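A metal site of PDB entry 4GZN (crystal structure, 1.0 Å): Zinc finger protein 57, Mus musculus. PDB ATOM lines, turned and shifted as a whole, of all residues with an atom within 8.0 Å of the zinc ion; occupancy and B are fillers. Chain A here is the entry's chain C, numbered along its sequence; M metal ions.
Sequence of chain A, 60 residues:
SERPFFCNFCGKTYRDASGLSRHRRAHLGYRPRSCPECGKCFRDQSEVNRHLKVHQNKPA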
ATOM      1  N   PHE A   6      21.731  -1.471  21.675  1.00  0.00           N
ATOM      2  CA  PHE A   6      22.401  -2.451  22.517  1.00  0.00           C
ATOM      3  C   PHE A   6      23.780  -2.031  22.966  1.00  0.00           C
ATOM      4  O   PHE A   6      24.481  -1.234  22.319  1.00  0.00           O
ATOM      5  CB  PHE A   6      22.437  -3.838  21.863  1.00  0.00           C
ATOM      6  CG  PHE A   6      23.366  -3.940  20.689  1.00  0.00           C
ATOM      7  CD1 PHE A   6      22.953  -3.549  19.432  1.00  0.00           C
ATOM      8  CD2 PHE A   6      24.667  -4.402  20.861  1.00  0.00           C
ATOM      9  CE1 PHE A   6      23.817  -3.629  18.361  1.00  0.00           C
ATOM     10  CE2 PHE A   6      25.524  -4.486  19.778  1.00  0.00           C
ATOM     11  CZ  PHE A   6      25.097  -4.103  18.539  1.00  0.00           C
ATOM     12  N   CYS A   7      24.156  -2.604  24.100  1.00  0.00           N
ATOM     13  CA  CYS A   7      25.439  -2.367  24.736  1.00  0.00           C
ATOM     14  C   CYS A   7      26.562  -3.158  24.085  1.00  0.00           C
ATOM     15  O   CYS A   7      26.425  -4.361  23.878  1.00  0.00           O
ATOM     16  CB  CYS A   7      25.325  -2.788  26.191  1.00  0.00           C
ATOM     17  SG  CYS A   7      26.851  -2.601  27.113  1.00  0.00           S
ATOM     18  N   ASN A   8      27.681  -2.499  23.791  1.00  0.00           N
ATOM     19  CA  ASN A   8      28.804  -3.158  23.131  1.00  0.00           C
ATOM     20  C   ASN A   8      29.715  -3.935  24.073  1.00  0.00           C
ATOM     21  O   ASN A   8      30.662  -4.579  23.609  1.00  0.00           O
ATOM     22  CB  ASN A   8      29.633  -2.160  22.316  1.00  0.00           C
ATOM     23  CG  ASN A   8      28.838  -1.504  21.195  1.00  0.00           C
ATOM     24  OD1 ASN A   8      28.011  -2.139  20.539  1.00  0.00           O
ATOM     25  ND2 ASN A   8      29.081  -0.221  20.989  1.00  0.00           N
ATOM     26  N   PHE A   9      29.399  -4.038  25.333  1.00  0.00           N
ATOM     27  CA  PHE A   9      30.246  -4.879  26.137  1.00  0.00           C
ATOM     28  C   PHE A   9      29.474  -6.032  26.739  1.00  0.00           C
ATOM     29  O   PHE A   9      30.075  -7.030  27.138  1.00  0.00           O
ATOM     30  CB  PHE A   9      30.864  -4.053  27.249  1.00  0.00           C
ATOM     31  CG  PHE A   9      31.803  -2.979  26.775  1.00  0.00           C
ATOM     32  CD1 PHE A   9      33.165  -3.212  26.700  1.00  0.00           C
ATOM     33  CD2 PHE A   9      31.323  -1.721  26.418  1.00  0.00           C
ATOM     34  CE1 PHE A   9      34.022  -2.231  26.277  1.00  0.00           C
ATOM     35  CE2 PHE A   9      32.188  -0.738  25.998  1.00  0.00           C
ATOM     36  CZ  PHE A   9      33.532  -0.993  25.930  1.00  0.00           C
ATOM     37  N   CYS A  10      28.149  -5.890  26.849  1.00  0.00           N
ATOM     38  CA  CYS A  10      27.390  -7.045  27.371  1.00  0.00           C
ATOM     39  C   CYS A  10      26.155  -7.400  26.567  1.00  0.00           C
ATOM     40  O   CYS A  10      25.457  -8.348  26.897  1.00  0.00           O
ATOM     41  CB  CYS A  10      26.989  -6.842  28.846  1.00  0.00           C
ATOM     42  SG  CYS A  10      25.538  -5.753  29.064  1.00  0.00           S
ATOM     43  N   GLY A  11      25.864  -6.615  25.523  1.00  0.00           N
ATOM     44  CA  GLY A  11      24.770  -6.959  24.624  1.00  0.00           C
ATOM     45  C   GLY A  11      23.367  -6.653  25.120  1.00  0.00           C
ATOM     46  O   GLY A  11      22.409  -6.944  24.415  1.00  0.00           O
ATOM     47  N   LYS A  12      23.214  -6.072  26.311  1.00  0.00           N
ATOM     48  CA  LYS A  12      21.869  -5.753  26.781  1.00  0.00           C
ATOM     49  C   LYS A  12      21.189  -4.808  25.814  1.00  0.00           C
ATOM     50  O   LYS A  12      21.787  -3.853  25.313  1.00  0.00           O
ATOM     51  CB  LYS A  12      21.875  -5.201  28.206  1.00  0.00           C
ATOM     52  CG  LYS A  12      21.656  -6.283  29.259  1.00  0.00           C
ATOM     53  CD  LYS A  12      21.816  -5.791  30.699  1.00  0.00           C
ATOM     54  CE  LYS A  12      20.822  -4.701  31.051  1.00  0.00           C
ATOM     55  NZ  LYS A  12      19.426  -5.175  30.986  1.00  0.00           N
ATOM     56  N   THR A  13      19.921  -5.087  25.549  1.00  0.00           N
ATOM     57  CA  THR A  13      19.163  -4.363  24.547  1.00  0.00           C
ATOM     58  C   THR A  13      18.130  -3.424  25.163  1.00  0.00           C
ATOM     59  O   THR A  13      17.678  -3.629  26.299  1.00  0.00           O
ATOM     60  CB  THR A  13      18.428  -5.328  23.597  1.00  0.00           C
ATOM     61  OG1 THR A  13      17.383  -5.988  24.327  1.00  0.00           O
ATOM     62  CG2 THR A  13      19.406  -6.360  23.009  1.00  0.00           C
ATOM     63  N   TYR A  14      17.751  -2.407  24.386  1.00  0.00           N
ATOM     64  CA  TYR A  14      16.882  -1.318  24.820  1.00  0.00           C
ATOM     65  C   TYR A  14      15.903  -0.916  23.721  1.00  0.00           C
ATOM     66  O   TYR A  14      16.211  -0.997  22.528  1.00  0.00           O
ATOM     67  CB  TYR A  14      17.733  -0.097  25.250  1.00  0.00           C
ATOM     68  CG  TYR A  14      18.463  -0.447  26.517  1.00  0.00           C
ATOM     69  CD1 TYR A  14      17.800  -0.375  27.737  1.00  0.00           C
ATOM     70  CD2 TYR A  14      19.739  -0.980  26.490  1.00  0.00           C
ATOM     71  CE1 TYR A  14      18.413  -0.789  28.902  1.00  0.00           C
ATOM     72  CE2 TYR A  14      20.373  -1.392  27.651  1.00  0.00           C
ATOM     73  CZ  TYR A  14      19.695  -1.307  28.843  1.00  0.00           C
ATOM     74  OH  TYR A  14      20.333  -1.754  29.978  1.00  0.00           O
ATOM     75  N   LEU A  20      19.815   2.830  26.868  1.00  0.00           N
ATOM     76  CA  LEU A  20      21.190   2.487  26.527  1.00  0.00           C
ATOM     77  C   LEU A  20      22.164   3.522  27.086  1.00  0.00           C
ATOM     78  O   LEU A  20      23.209   3.179  27.626  1.00  0.00           O
ATOM     79  CB  LEU A  20      21.351   2.329  25.013  1.00  0.00           C
ATOM     80  CG  LEU A  20      22.779   2.026  24.577  1.00  0.00           C
ATOM     81  CD1 LEU A  20      23.310   0.738  25.176  1.00  0.00           C
ATOM     82  CD2 LEU A  20      22.882   1.981  23.048  1.00  0.00           C
ATOM     83  N   HIS A  23      22.519   2.846  30.718  1.00  0.00           N
ATOM     84  CA  HIS A  23      23.208   1.596  30.970  1.00  0.00           C
ATOM     85  C   HIS A  23      24.711   1.738  30.726  1.00  0.00           C
ATOM     86  O   HIS A  23      25.523   1.271  31.528  1.00  0.00           O
ATOM     87  CB  HIS A  23      22.592   0.523  30.074  1.00  0.00           C
ATOM     88  CG  HIS A  23      23.305  -0.787  30.100  1.00  0.00           C
ATOM     89  ND1 HIS A  23      23.122  -1.723  31.089  1.00  0.00           N
ATOM     90  CD2 HIS A  23      24.217  -1.314  29.247  1.00  0.00           C
ATOM     91  CE1 HIS A  23      23.885  -2.769  30.848  1.00  0.00           C
ATOM     92  NE2 HIS A  23      24.560  -2.553  29.738  1.00  0.00           N
ATOM     93  N   ARG A  24      25.089   2.369  29.620  1.00  0.00           N
ATOM     94  CA  ARG A  24      26.503   2.605  29.334  1.00  0.00           C
ATOM     95  C   ARG A  24      27.157   3.396  30.452  1.00  0.00           C
ATOM     96  O   ARG A  24      28.256   3.065  30.912  1.00  0.00           O
ATOM     97  CB  ARG A  24      26.689   3.390  28.029  1.00  0.00           C
ATOM     98  CG  ARG A  24      26.334   2.686  26.738  1.00  0.00           C
ATOM     99  CD  ARG A  24      26.559   3.627  25.528  1.00  0.00           C
ATOM    100  NE  ARG A  24      25.864   4.913  25.639  1.00  0.00           N
ATOM    101  CZ  ARG A  24      25.404   5.617  24.607  1.00  0.00           C
ATOM    102  NH1 ARG A  24      24.777   6.786  24.810  1.00  0.00           N
ATOM    103  NH2 ARG A  24      25.557   5.162  23.377  1.00  0.00           N
ATOM    104  N   ALA A  26      26.225   3.590  33.507  1.00  0.00           N
ATOM    105  CA  ALA A  26      26.302   2.756  34.702  1.00  0.00           C
ATOM    106  C   ALA A  26      27.545   1.847  34.656  1.00  0.00           C
ATOM    107  O   ALA A  26      28.245   1.689  35.653  1.00  0.00           O
ATOM    108  CB  ALA A  26      25.014   1.956  34.899  1.00  0.00           C
ATOM    109  N   HIS A  27      27.841   1.248  33.493  1.00  0.00           N
ATOM    110  CA  HIS A  27      29.095   0.493  33.385  1.00  0.00           C
ATOM    111  C   HIS A  27      30.296   1.403  33.675  1.00  0.00           C
ATOM    112  O   HIS A  27      31.277   0.946  34.253  1.00  0.00           O
ATOM    113  CB  HIS A  27      29.332  -0.077  31.976  1.00  0.00           C
ATOM    114  CG  HIS A  27      28.561  -1.318  31.607  1.00  0.00           C
ATOM    115  ND1 HIS A  27      28.659  -2.525  32.269  1.00  0.00           N
ATOM    116  CD2 HIS A  27      27.803  -1.564  30.513  1.00  0.00           C
ATOM    117  CE1 HIS A  27      27.951  -3.439  31.628  1.00  0.00           C
ATOM    118  NE2 HIS A  27      27.415  -2.886  30.552  1.00  0.00           N
HETATM  119 ZN    ZN M   1      26.210  -3.603  29.100  1.00  0.00          ZN
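The zinc ion is bound by NE2 of His 27, 2.0 Å away. The zinc ion is bound by NE2 of His 23, at 2.1 Å. The zinc ion is bound by SG of Cys 10 (2.3 Å). The zinc ion is bound by the side-chain sulfur (SG) of Cys 7.
Of the 14 residues printed, 4 come within 4 Å of the zinc ion. Along chain A the residues within 4 Å of the zinc ion span positions 7 to 27. The nearest printed residue that does not touch the zinc ion is Gly 11 (4.7 Å).
N of Cys 7 is in hydrogen-bond range of O of Lys 12. The backbone NH (N) of Phe 9 sits close to the side-chain sulfur (SG) of Cys 7 (3.4 Å). SG of Cys 10 lies close to N of Lys 12 (3.6 Å). A ring nitrogen (ND1) of His 23 lies within hydrogen-bond range of the side-chain hydroxyl (OH) of Tyr 14 (3.0 Å).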
